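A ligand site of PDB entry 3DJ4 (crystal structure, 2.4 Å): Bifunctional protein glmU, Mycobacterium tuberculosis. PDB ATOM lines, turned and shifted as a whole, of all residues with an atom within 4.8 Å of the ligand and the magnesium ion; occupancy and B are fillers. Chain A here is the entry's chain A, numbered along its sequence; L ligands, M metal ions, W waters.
The side-chain amide oxygen (OD1) of Asn 239 sits close to the side-chain amino group (NZ) of Lys 26, at 3.0 Å.
The backbone NH of Val 238 lies within hydrogen-bond range of the backbone carbonyl oxygen of Asp 114 (3.0 Å).
O of Gly 151 is in hydrogen-bond range of N of Asn 181 (2.9 Å).
The side-chain amide oxygen (OD1) of Asn 181 sits at hydrogen-bond distance from the backbone NH (N) of Gly 183 (3.0 Å).
The backbone carbonyl oxygen (O) of Leu 12 is in hydrogen-bond range of the backbone NH (N) of Gly 113 (3.0 Å).
NE2 of Gln 83 is in hydrogen-bond range of O of Gly 88 (3.3 Å).
The side-chain amino group (NZ) of Lys 26 sits close to the backbone carbonyl oxygen (O) of Val 238 (3.5 Å).
N of Ala 13 is in hydrogen-bond range of O of Val 55 (2.9 Å).
The backbone carbonyl oxygen (O) of Asn 181 is in hydrogen-bond range of an oxygen (O3) of the ligand, 2.7 Å away.
The side-chain amide nitrogen (ND2) of Asn 181 is in hydrogen-bond range of an oxygen (O2) of the ligand (2.7 Å).
OG1 of Thr 89 sits at hydrogen-bond distance from O6 of the ligand (2.7 Å).
N1 of the ligand is in hydrogen-bond range of OE1 of Glu 166, at 2.9 Å.
The backbone carbonyl oxygen of Leu 12 sits at hydrogen-bond distance from an oxygen (O11) of the ligand.
N of Ala 14 sits at hydrogen-bond distance from O7 of the ligand (2.9 Å).
A nitrogen (N3) of the ligand is in hydrogen-bond range of the side-chain amide oxygen (OE1) of Gln 83 (3.0 Å).
O3 of the ligand sits at hydrogen-bond distance from N of Gly 151, 3.0 Å away.
The backbone NH (N) of Gly 15 lies within hydrogen-bond range of an oxygen (O9) of the ligand, 3.1 Å away.
An oxygen (O8) of the ligand lies within hydrogen-bond range of the backbone NH (N) of Gly 88, at 3.1 Å.
The side-chain amino group (NZ) of Lys 26 lies close to an oxygen (O14) of the ligand, 3.1 Å away.
The backbone NH (N) of Gly 113 sits at hydrogen-bond distance from an oxygen (O11) of the ligand (3.3 Å).
OD1 of Asn 239 is bound to the magnesium ion (2.0 Å).
The magnesium ion is bound by O16 of the ligand.
OD2 of Asp 114 binds the magnesium ion (2.0 Å).
The magnesium ion is bound by water W6.
An oxygen (O14) of the ligand binds the magnesium ion (2.1 Å).
Water W2 binds the magnesium ion, at 2.3 Å.
The magnesium ion has six donor atoms within binding distance.
Water W6 lies within hydrogen-bond range of the side-chain carboxylate (OD1) of Asp 114 (2.7 Å) and an oxygen (O5) of the ligand (3.0 Å).
Water W2 lies within hydrogen-bond range of an oxygen (O5) of the ligand, the backbone NH (N) of Val 238 and the side-chain amide nitrogen (ND2) of Asn 239.
Water W3 lies within hydrogen-bond range of O17 of the ligand, O of Gly 149 and ND2 of Asn 239.
Water W5 lies within hydrogen-bond range of OH of Tyr 185 and O6 of the ligand.
Water W4 lies within hydrogen-bond range of the backbone carbonyl oxygen (O) of Ala 182 (2.6 Å), the side-chain hydroxyl (OG1) of Thr 115 (2.6 Å) and an oxygen (O5) of the ligand (2.8 Å).
Water W1 bridges NH2 of Arg 19 (3.0 Å) and O13 of the ligand (3.3 Å).
Lys 26 touches the magnesium ion.
Of the 33 residues printed, 3 come within 4 Å of the magnesium ion.
Along chain A the residues within 4 Å of the magnesium ion span positions 26 to 239.
Ala 13 touches the ligand.
CA of Pro 86 touches O8 of the ligand (3.1 Å).
Leu 87 touches the ligand (N to O8, 3.6 Å).
Ala 92 touches the ligand (CB to O7, 3.5 Å).
Ser 112 touches the ligand (OG to C16, 3.5 Å).
CD1 of Tyr 150 touches O3 of the ligand, at 3.4 Å.
Ala 182 touches the ligand (O to C6, 3.6 Å).
Tyr 209 touches the ligand (CD1 to C8, 3.8 Å).
Thr 211 touches the ligand.
Gly 237 touches the ligand (CA to O5, 3.9 Å).
Hydrophobic or aromatic side chains that line the ligand: Leu 12, Ala 14, Pro 86, Ala 92, Tyr 150 and Tyr 209.
23 residues have an atom within 4 Å of the ligand: Leu 12, Ala 13, Ala 14, Gly 15, Lys 26, Gln 83, Pro 86, Leu 87, Gly 88, Thr 89, Ala 92, Ser 112, Gly 113, Asp 114, Tyr 150, Gly 151, Glu 166, Asn 181, Ala 182, Tyr 209, Thr 211, Gly 237 and Asn 239.
The nearest printed residue that does not touch the ligand is Gly 149 (4.04 Å).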
ATOM      1  N   LEU A  12      15.301   2.053 -13.375  1.00  0.00           N
ATOM      2  CA  LEU A  12      16.109   1.183 -12.532  1.00  0.00           C
ATOM      3  C   LEU A  12      15.803  -0.289 -12.816  1.00  0.00           C
ATOM      4  O   LEU A  12      14.699  -0.764 -12.556  1.00  0.00           O
ATOM      5  CB  LEU A  12      15.884   1.487 -11.052  1.00  0.00           C
ATOM      6  CG  LEU A  12      16.005   2.957 -10.645  1.00  0.00           C
ATOM      7  CD1 LEU A  12      15.849   3.111  -9.140  1.00  0.00           C
ATOM      8  CD2 LEU A  12      17.338   3.531 -11.110  1.00  0.00           C
ATOM      9  N   ALA A  13      16.791  -1.003 -13.344  1.00  0.00           N
ATOM     10  CA  ALA A  13      16.571  -2.347 -13.870  1.00  0.00           C
ATOM     11  C   ALA A  13      17.711  -3.281 -13.480  1.00  0.00           C
ATOM     12  O   ALA A  13      18.058  -4.186 -14.240  1.00  0.00           O
ATOM     13  CB  ALA A  13      16.400  -2.301 -15.379  1.00  0.00           C
ATOM     14  N   ALA A  14      18.283  -3.061 -12.306  1.00  0.00           N
ATOM     15  CA  ALA A  14      19.563  -3.644 -11.956  1.00  0.00           C
ATOM     16  C   ALA A  14      19.424  -4.660 -10.817  1.00  0.00           C
ATOM     17  O   ALA A  14      20.401  -5.294 -10.429  1.00  0.00           O
ATOM     18  CB  ALA A  14      20.561  -2.558 -11.571  1.00  0.00           C
ATOM     19  N   GLY A  15      18.207  -4.790 -10.303  1.00  0.00           N
ATOM     20  CA  GLY A  15      17.942  -5.685  -9.206  1.00  0.00           C
ATOM     21  C   GLY A  15      18.132  -7.131  -9.573  1.00  0.00           C
ATOM     22  O   GLY A  15      18.127  -7.495 -10.748  1.00  0.00           O
ATOM     23  N   ARG A  19      12.346 -12.976  -6.414  1.00  0.00           N
ATOM     24  CA  ARG A  19      11.047 -13.641  -6.156  1.00  0.00           C
ATOM     25  C   ARG A  19      10.334 -14.105  -7.393  1.00  0.00           C
ATOM     26  O   ARG A  19       9.264 -14.739  -7.310  1.00  0.00           O
ATOM     27  CB  ARG A  19      10.182 -12.798  -5.236  1.00  0.00           C
ATOM     28  CG  ARG A  19      10.649 -12.895  -3.748  1.00  0.00           C
ATOM     29  CD  ARG A  19      10.176 -11.698  -2.947  1.00  0.00           C
ATOM     30  NE  ARG A  19      10.369 -10.400  -3.654  1.00  0.00           N
ATOM     31  CZ  ARG A  19      11.266  -9.449  -3.290  1.00  0.00           C
ATOM     32  NH1 ARG A  19      12.051  -9.671  -2.208  1.00  0.00           N
ATOM     33  NH2 ARG A  19      11.367  -8.293  -3.985  1.00  0.00           N
ATOM     34  N   LYS A  26      14.012 -10.313 -14.566  1.00  0.00           N
ATOM     35  CA  LYS A  26      12.647  -9.920 -14.262  1.00  0.00           C
ATOM     36  C   LYS A  26      12.058  -8.950 -15.301  1.00  0.00           C
ATOM     37  O   LYS A  26      10.911  -9.092 -15.794  1.00  0.00           O
ATOM     38  CB  LYS A  26      12.614  -9.289 -12.868  1.00  0.00           C
ATOM     39  CG  LYS A  26      11.278  -8.535 -12.604  1.00  0.00           C
ATOM     40  CD  LYS A  26      11.003  -8.412 -11.132  1.00  0.00           C
ATOM     41  CE  LYS A  26      11.444  -7.117 -10.584  1.00  0.00           C
ATOM     42  NZ  LYS A  26      11.173  -7.039  -9.220  1.00  0.00           N
ATOM     43  N   VAL A  27      12.862  -7.945 -15.633  1.00  0.00           N
ATOM     44  CA  VAL A  27      12.459  -6.876 -16.515  1.00  0.00           C
ATOM     45  C   VAL A  27      12.189  -7.341 -17.947  1.00  0.00           C
ATOM     46  O   VAL A  27      11.580  -6.609 -18.726  1.00  0.00           O
ATOM     47  CB  VAL A  27      13.466  -5.742 -16.407  1.00  0.00           C
ATOM     48  CG1 VAL A  27      13.133  -4.700 -17.367  1.00  0.00           C
ATOM     49  CG2 VAL A  27      13.385  -5.106 -15.003  1.00  0.00           C
ATOM     50  N   VAL A  55      19.587   1.817 -15.883  1.00  0.00           N
ATOM     51  CA  VAL A  55      20.538   1.269 -14.922  1.00  0.00           C
ATOM     52  C   VAL A  55      20.438  -0.238 -14.986  1.00  0.00           C
ATOM     53  O   VAL A  55      19.366  -0.806 -14.666  1.00  0.00           O
ATOM     54  CB  VAL A  55      20.236   1.753 -13.479  1.00  0.00           C
ATOM     55  CG1 VAL A  55      21.226   1.248 -12.491  1.00  0.00           C
ATOM     56  CG2 VAL A  55      20.159   3.323 -13.411  1.00  0.00           C
ATOM     57  N   GLN A  83      25.506  -0.691 -12.584  1.00  0.00           N
ATOM     58  CA  GLN A  83      25.593  -0.812 -11.129  1.00  0.00           C
ATOM     59  C   GLN A  83      25.976  -2.266 -10.864  1.00  0.00           C
ATOM     60  O   GLN A  83      25.150  -3.180 -11.012  1.00  0.00           O
ATOM     61  CB  GLN A  83      24.245  -0.484 -10.474  1.00  0.00           C
ATOM     62  CG  GLN A  83      24.262  -0.514  -8.928  1.00  0.00           C
ATOM     63  CD  GLN A  83      22.893  -0.782  -8.288  1.00  0.00           C
ATOM     64  OE1 GLN A  83      22.076  -1.504  -8.873  1.00  0.00           O
ATOM     65  NE2 GLN A  83      22.657  -0.248  -7.068  1.00  0.00           N
ATOM     66  N   PRO A  86      23.944  -4.939  -6.531  1.00  0.00           N
ATOM     67  CA  PRO A  86      22.657  -4.412  -6.158  1.00  0.00           C
ATOM     68  C   PRO A  86      22.572  -4.011  -4.692  1.00  0.00           C
ATOM     69  O   PRO A  86      21.879  -4.656  -3.883  1.00  0.00           O
ATOM     70  CB  PRO A  86      21.703  -5.542  -6.508  1.00  0.00           C
ATOM     71  CG  PRO A  86      22.583  -6.783  -6.307  1.00  0.00           C
ATOM     72  CD  PRO A  86      23.921  -6.389  -6.741  1.00  0.00           C
ATOM     73  N   LEU A  87      23.222  -2.884  -4.398  1.00  0.00           N
ATOM     74  CA  LEU A  87      23.295  -2.317  -3.067  1.00  0.00           C
ATOM     75  C   LEU A  87      22.028  -1.570  -2.657  1.00  0.00           C
ATOM     76  O   LEU A  87      21.879  -1.192  -1.510  1.00  0.00           O
ATOM     77  CB  LEU A  87      24.561  -1.462  -2.946  1.00  0.00           C
ATOM     78  CG  LEU A  87      25.949  -2.154  -2.782  1.00  0.00           C
ATOM     79  CD1 LEU A  87      26.420  -2.699  -4.033  1.00  0.00           C
ATOM     80  CD2 LEU A  87      27.060  -1.204  -2.345  1.00  0.00           C
ATOM     81  N   GLY A  88      21.102  -1.353  -3.575  1.00  0.00           N
ATOM     82  CA  GLY A  88      19.845  -0.650  -3.246  1.00  0.00           C
ATOM     83  C   GLY A  88      19.385   0.331  -4.311  1.00  0.00           C
ATOM     84  O   GLY A  88      20.180   0.720  -5.172  1.00  0.00           O
ATOM     85  N   THR A  89      18.099   0.732  -4.231  1.00  0.00           N
ATOM     86  CA  THR A  89      17.455   1.611  -5.222  1.00  0.00           C
ATOM     87  C   THR A  89      18.043   3.026  -5.158  1.00  0.00           C
ATOM     88  O   THR A  89      18.158   3.693  -6.200  1.00  0.00           O
ATOM     89  CB  THR A  89      15.896   1.643  -5.111  1.00  0.00           C
ATOM     90  OG1 THR A  89      15.522   1.963  -3.739  1.00  0.00           O
ATOM     91  CG2 THR A  89      15.225   0.260  -5.491  1.00  0.00           C
ATOM     92  N   ALA A  92      21.273   2.416  -6.891  1.00  0.00           N
ATOM     93  CA  ALA A  92      20.992   2.410  -8.334  1.00  0.00           C
ATOM     94  C   ALA A  92      20.907   3.815  -8.888  1.00  0.00           C
ATOM     95  O   ALA A  92      21.445   4.036  -9.934  1.00  0.00           O
ATOM     96  CB  ALA A  92      19.730   1.658  -8.659  1.00  0.00           C
ATOM     97  N   SER A 112      10.804   2.436 -12.047  1.00  0.00           N
ATOM     98  CA  SER A 112      11.297   1.061 -11.883  1.00  0.00           C
ATOM     99  C   SER A 112      11.066   0.358 -13.224  1.00  0.00           C
ATOM    100  O   SER A 112      10.138   0.720 -13.971  1.00  0.00           O
ATOM    101  CB  SER A 112      10.533   0.283 -10.769  1.00  0.00           C
ATOM    102  OG  SER A 112      10.748   0.795  -9.472  1.00  0.00           O
ATOM    103  N   GLY A 113      11.904  -0.613 -13.553  1.00  0.00           N
ATOM    104  CA  GLY A 113      11.654  -1.387 -14.789  1.00  0.00           C
ATOM    105  C   GLY A 113      10.509  -2.322 -14.542  1.00  0.00           C
ATOM    106  O   GLY A 113       9.988  -2.926 -15.475  1.00  0.00           O
ATOM    107  N   ASP A 114      10.047  -2.398 -13.290  1.00  0.00           N
ATOM    108  CA  ASP A 114       8.974  -3.407 -12.963  1.00  0.00           C
ATOM    109  C   ASP A 114       7.548  -2.865 -12.707  1.00  0.00           C
ATOM    110  O   ASP A 114       6.768  -3.525 -12.082  1.00  0.00           O
ATOM    111  CB  ASP A 114       9.430  -4.373 -11.819  1.00  0.00           C
ATOM    112  CG  ASP A 114       9.391  -3.732 -10.474  1.00  0.00           C
ATOM    113  OD1 ASP A 114       9.131  -2.467 -10.508  1.00  0.00           O
ATOM    114  OD2 ASP A 114       9.609  -4.464  -9.431  1.00  0.00           O
ATOM    115  N   THR A 115       7.260  -1.654 -13.196  1.00  0.00           N
ATOM    116  CA  THR A 115       5.924  -1.020 -13.218  1.00  0.00           C
ATOM    117  C   THR A 115       5.455  -0.853 -14.686  1.00  0.00           C
ATOM    118  O   THR A 115       5.596   0.234 -15.271  1.00  0.00           O
ATOM    119  CB  THR A 115       6.026   0.383 -12.468  1.00  0.00           C
ATOM    120  OG1 THR A 115       6.447   0.135 -11.120  1.00  0.00           O
ATOM    121  CG2 THR A 115       4.702   1.130 -12.394  1.00  0.00           C
ATOM    122  N   GLY A 149       4.240  -5.638   0.467  1.00  0.00           N
ATOM    123  CA  GLY A 149       5.432  -5.486  -0.338  1.00  0.00           C
ATOM    124  C   GLY A 149       5.765  -4.064  -0.750  1.00  0.00           C
ATOM    125  O   GLY A 149       6.906  -3.770  -1.115  1.00  0.00           O
ATOM    126  N   TYR A 150       4.776  -3.179  -0.657  1.00  0.00           N
ATOM    127  CA  TYR A 150       4.924  -1.765  -0.969  1.00  0.00           C
ATOM    128  C   TYR A 150       5.419  -0.991   0.255  1.00  0.00           C
ATOM    129  O   TYR A 150       5.132  -1.366   1.406  1.00  0.00           O
ATOM    130  CB  TYR A 150       3.557  -1.131  -1.424  1.00  0.00           C
ATOM    131  CG  TYR A 150       3.054  -1.510  -2.833  1.00  0.00           C
ATOM    132  CD1 TYR A 150       3.437  -0.779  -3.987  1.00  0.00           C
ATOM    133  CD2 TYR A 150       2.179  -2.595  -3.012  1.00  0.00           C
ATOM    134  CE1 TYR A 150       2.976  -1.105  -5.267  1.00  0.00           C
ATOM    135  CE2 TYR A 150       1.734  -2.952  -4.302  1.00  0.00           C
ATOM    136  CZ  TYR A 150       2.130  -2.203  -5.401  1.00  0.00           C
ATOM    137  OH  TYR A 150       1.677  -2.620  -6.617  1.00  0.00           O
ATOM    138  N   GLY A 151       6.122   0.112  -0.001  1.00  0.00           N
ATOM    139  CA  GLY A 151       6.550   0.978   1.047  1.00  0.00           C
ATOM    140  C   GLY A 151       5.345   1.814   1.320  1.00  0.00           C
ATOM    141  O   GLY A 151       4.703   2.282   0.379  1.00  0.00           O
ATOM    142  N   ILE A 164       8.747   7.538   3.717  1.00  0.00           N
ATOM    143  CA  ILE A 164       8.267   6.248   3.220  1.00  0.00           C
ATOM    144  C   ILE A 164       8.907   5.098   4.050  1.00  0.00           C
ATOM    145  O   ILE A 164      10.137   5.108   4.291  1.00  0.00           O
ATOM    146  CB  ILE A 164       8.555   6.067   1.761  1.00  0.00           C
ATOM    147  CG1 ILE A 164       7.811   7.141   0.953  1.00  0.00           C
ATOM    148  CG2 ILE A 164       8.188   4.588   1.280  1.00  0.00           C
ATOM    149  CD1 ILE A 164       8.316   7.272  -0.453  1.00  0.00           C
ATOM    150  N   GLU A 166       9.499   0.878   4.254  1.00  0.00           N
ATOM    151  CA  GLU A 166       9.437  -0.421   3.588  1.00  0.00           C
ATOM    152  C   GLU A 166       8.670  -1.542   4.347  1.00  0.00           C
ATOM    153  O   GLU A 166       8.665  -1.576   5.545  1.00  0.00           O
ATOM    154  CB  GLU A 166      10.861  -0.912   3.130  1.00  0.00           C
ATOM    155  CG  GLU A 166      11.488  -0.048   2.107  1.00  0.00           C
ATOM    156  CD  GLU A 166      10.616   0.254   0.947  1.00  0.00           C
ATOM    157  OE1 GLU A 166      10.387  -0.669   0.134  1.00  0.00           O
ATOM    158  OE2 GLU A 166      10.155   1.437   0.845  1.00  0.00           O
ATOM    159  N   ASN A 181       3.594   3.598  -1.984  1.00  0.00           N
ATOM    160  CA  ASN A 181       4.589   4.260  -2.816  1.00  0.00           C
ATOM    161  C   ASN A 181       4.616   3.613  -4.173  1.00  0.00           C
ATOM    162  O   ASN A 181       4.846   2.393  -4.278  1.00  0.00           O
ATOM    163  CB  ASN A 181       6.006   4.099  -2.154  1.00  0.00           C
ATOM    164  CG  ASN A 181       7.136   4.690  -2.983  1.00  0.00           C
ATOM    165  OD1 ASN A 181       6.943   5.626  -3.789  1.00  0.00           O
ATOM    166  ND2 ASN A 181       8.350   4.172  -2.773  1.00  0.00           N
ATOM    167  N   ALA A 182       4.427   4.419  -5.216  1.00  0.00           N
ATOM    168  CA  ALA A 182       4.419   3.942  -6.604  1.00  0.00           C
ATOM    169  C   ALA A 182       5.820   3.593  -7.068  1.00  0.00           C
ATOM    170  O   ALA A 182       5.966   2.787  -8.006  1.00  0.00           O
ATOM    171  CB  ALA A 182       3.795   5.000  -7.566  1.00  0.00           C
ATOM    172  N   GLY A 183       6.843   4.198  -6.435  1.00  0.00           N
ATOM    173  CA  GLY A 183       8.210   4.039  -6.866  1.00  0.00           C
ATOM    174  C   GLY A 183       8.532   4.943  -8.060  1.00  0.00           C
ATOM    175  O   GLY A 183       9.465   4.685  -8.823  1.00  0.00           O
ATOM    176  N   TYR A 185       9.152   8.962  -9.277  1.00  0.00           N
ATOM    177  CA  TYR A 185       9.462  10.266  -8.653  1.00  0.00           C
ATOM    178  C   TYR A 185       9.939  11.332  -9.606  1.00  0.00           C
ATOM    179  O   TYR A 185      10.607  11.032 -10.633  1.00  0.00           O
ATOM    180  CB  TYR A 185      10.585  10.123  -7.595  1.00  0.00           C
ATOM    181  CG  TYR A 185      10.620   8.875  -6.666  1.00  0.00           C
ATOM    182  CD1 TYR A 185      11.000   7.628  -7.146  1.00  0.00           C
ATOM    183  CD2 TYR A 185      10.309   8.980  -5.310  1.00  0.00           C
ATOM    184  CE1 TYR A 185      11.058   6.515  -6.296  1.00  0.00           C
ATOM    185  CE2 TYR A 185      10.326   7.835  -4.459  1.00  0.00           C
ATOM    186  CZ  TYR A 185      10.739   6.625  -4.960  1.00  0.00           C
ATOM    187  OH  TYR A 185      10.787   5.513  -4.101  1.00  0.00           O
ATOM    188  N   TYR A 209      18.343   2.467   0.500  1.00  0.00           N
ATOM    189  CA  TYR A 209      16.963   2.670  -0.040  1.00  0.00           C
ATOM    190  C   TYR A 209      16.728   4.043  -0.730  1.00  0.00           C
ATOM    191  O   TYR A 209      16.981   5.056  -0.118  1.00  0.00           O
ATOM    192  CB  TYR A 209      15.976   2.635   1.177  1.00  0.00           C
ATOM    193  CG  TYR A 209      15.759   1.342   1.954  1.00  0.00           C
ATOM    194  CD1 TYR A 209      15.988   0.083   1.389  1.00  0.00           C
ATOM    195  CD2 TYR A 209      15.254   1.375   3.248  1.00  0.00           C
ATOM    196  CE1 TYR A 209      15.714  -1.132   2.111  1.00  0.00           C
ATOM    197  CE2 TYR A 209      15.007   0.159   3.979  1.00  0.00           C
ATOM    198  CZ  TYR A 209      15.237  -1.055   3.377  1.00  0.00           C
ATOM    199  OH  TYR A 209      15.006  -2.247   4.026  1.00  0.00           O
ATOM    200  N   LEU A 210      16.184   4.128  -1.936  1.00  0.00           N
ATOM    201  CA  LEU A 210      15.768   5.459  -2.481  1.00  0.00           C
ATOM    202  C   LEU A 210      14.690   6.157  -1.633  1.00  0.00           C
ATOM    203  O   LEU A 210      14.573   7.429  -1.580  1.00  0.00           O
ATOM    204  CB  LEU A 210      15.186   5.361  -3.879  1.00  0.00           C
ATOM    205  CG  LEU A 210      14.927   6.687  -4.643  1.00  0.00           C
ATOM    206  CD1 LEU A 210      16.076   7.689  -4.624  1.00  0.00           C
ATOM    207  CD2 LEU A 210      14.564   6.317  -6.086  1.00  0.00           C
ATOM    208  N   THR A 211      13.878   5.327  -0.956  1.00  0.00           N
ATOM    209  CA  THR A 211      12.765   5.817  -0.184  1.00  0.00           C
ATOM    210  C   THR A 211      13.108   6.805   0.965  1.00  0.00           C
ATOM    211  O   THR A 211      12.255   7.671   1.378  1.00  0.00           O
ATOM    212  CB  THR A 211      11.932   4.618   0.316  1.00  0.00           C
ATOM    213  OG1 THR A 211      12.784   3.615   0.936  1.00  0.00           O
ATOM    214  CG2 THR A 211      11.236   4.041  -0.821  1.00  0.00           C
ATOM    215  N   GLY A 237       3.323  -2.472  -9.169  1.00  0.00           N
ATOM    216  CA  GLY A 237       4.559  -3.209  -9.356  1.00  0.00           C
ATOM    217  C   GLY A 237       4.429  -4.712  -9.551  1.00  0.00           C
ATOM    218  O   GLY A 237       3.432  -5.342  -9.158  1.00  0.00           O
ATOM    219  N   VAL A 238       5.465  -5.321 -10.126  1.00  0.00           N
ATOM    220  CA  VAL A 238       5.536  -6.774 -10.347  1.00  0.00           C
ATOM    221  C   VAL A 238       6.835  -7.327  -9.764  1.00  0.00           C
ATOM    222  O   VAL A 238       7.914  -7.200 -10.381  1.00  0.00           O
ATOM    223  CB  VAL A 238       5.441  -7.142 -11.850  1.00  0.00           C
ATOM    224  CG1 VAL A 238       5.803  -8.668 -12.062  1.00  0.00           C
ATOM    225  CG2 VAL A 238       4.048  -6.793 -12.383  1.00  0.00           C
ATOM    226  N   ASN A 239       6.705  -7.983  -8.589  1.00  0.00           N
ATOM    227  CA  ASN A 239       7.856  -8.606  -7.897  1.00  0.00           C
ATOM    228  C   ASN A 239       7.873 -10.123  -7.933  1.00  0.00           C
ATOM    229  O   ASN A 239       8.871 -10.737  -7.557  1.00  0.00           O
ATOM    230  CB  ASN A 239       7.999  -8.174  -6.433  1.00  0.00           C
ATOM    231  CG  ASN A 239       8.491  -6.677  -6.265  1.00  0.00           C
ATOM    232  OD1 ASN A 239       9.114  -6.110  -7.174  1.00  0.00           O
ATOM    233  ND2 ASN A 239       8.239  -6.080  -5.115  1.00  0.00           N
HETATM  234  C1  LIG L   1      10.117  -0.582  -4.484  1.00  0.00           C
HETATM  235  C2  LIG L   1      10.165   0.528  -3.452  1.00  0.00           C
HETATM  236  C3  LIG L   1       8.806   0.541  -2.710  1.00  0.00           C
HETATM  237  C4  LIG L   1       7.650   0.697  -3.668  1.00  0.00           C
HETATM  238  C5  LIG L   1       7.735  -0.302  -4.822  1.00  0.00           C
HETATM  239  C6  LIG L   1       6.610  -0.095  -5.880  1.00  0.00           C
HETATM  240  C7  LIG L   1      12.462   0.913  -2.560  1.00  0.00           C
HETATM  241  C8  LIG L   1      13.408   0.685  -1.402  1.00  0.00           C
HETATM  242  N1  LIG L   1      11.229   0.301  -2.460  1.00  0.00           N
HETATM  243  O1  LIG L   1       9.852  -1.768  -3.757  1.00  0.00           O
HETATM  244  O2  LIG L   1       8.696   1.660  -1.849  1.00  0.00           O
HETATM  245  O3  LIG L   1       6.405   0.639  -2.969  1.00  0.00           O
HETATM  246  O4  LIG L   1       9.072  -0.355  -5.443  1.00  0.00           O
HETATM  247  O5  LIG L   1       6.728  -1.149  -6.859  1.00  0.00           O
HETATM  248  O6  LIG L   1      12.812   1.655  -3.506  1.00  0.00           O
HETATM  249  N2  LIG L   1      16.852  -2.096  -8.532  1.00  0.00           N
HETATM  250  C9  LIG L   1      18.139  -1.698  -8.970  1.00  0.00           C
HETATM  251  N3  LIG L   1      19.208  -1.908  -8.139  1.00  0.00           N
HETATM  252  C10 LIG L   1      19.069  -2.491  -6.920  1.00  0.00           C
HETATM  253  C11 LIG L   1      17.783  -2.873  -6.482  1.00  0.00           C
HETATM  254  C12 LIG L   1      16.703  -2.668  -7.326  1.00  0.00           C
HETATM  255  O7  LIG L   1      18.341  -1.169 -10.099  1.00  0.00           O
HETATM  256  O8  LIG L   1      20.091  -2.649  -6.224  1.00  0.00           O
HETATM  257  C13 LIG L   1      15.655  -1.882  -9.403  1.00  0.00           C
HETATM  258  C14 LIG L   1      14.859  -3.168  -9.659  1.00  0.00           C
HETATM  259  O9  LIG L   1      15.324  -3.780 -10.843  1.00  0.00           O
HETATM  260  C15 LIG L   1      13.381  -2.725  -9.708  1.00  0.00           C
HETATM  261  C16 LIG L   1      13.338  -1.429  -8.935  1.00  0.00           C
HETATM  262  O10 LIG L   1      14.687  -1.038  -8.752  1.00  0.00           O
HETATM  263  O11 LIG L   1      12.957  -2.535 -11.062  1.00  0.00           O
HETATM  264  C17 LIG L   1      12.775  -1.473  -7.512  1.00  0.00           C
HETATM  265  O12 LIG L   1      13.357  -2.577  -6.830  1.00  0.00           O
HETATM  266  P1  LIG L   1      12.383  -3.875  -6.208  1.00  0.00           P
HETATM  267  O13 LIG L   1      13.339  -4.945  -5.556  1.00  0.00           O
HETATM  268  O14 LIG L   1      11.509  -4.542  -7.373  1.00  0.00           O
HETATM  269  O15 LIG L   1      11.913  -2.889  -4.618  1.00  0.00           O
HETATM  270  P2  LIG L   1      10.386  -3.178  -4.178  1.00  0.00           P
HETATM  271  O16 LIG L   1      10.339  -3.720  -5.709  1.00  0.00           O
HETATM  272  O17 LIG L   1      10.417  -4.234  -3.064  1.00  0.00           O
HETATM  273 MG    MG M   1       9.455  -4.178  -7.424  1.00  0.00          MG
HETATM  274  O   HOH W   1      12.984  -6.225  -2.555  1.00  0.00           O
HETATM  275  O   HOH W   2       7.129  -3.960  -7.548  1.00  0.00           O
HETATM  276  O   HOH W   3       8.892  -5.583  -1.727  1.00  0.00           O
HETATM  277  O   HOH W   4       5.345   0.359  -8.753  1.00  0.00           O
HETATM  278  O   HOH W   5      11.850   3.624  -5.187  1.00  0.00           O
HETATM  279  O   HOH W   6       9.378  -2.148  -7.830  1.00  0.00           O
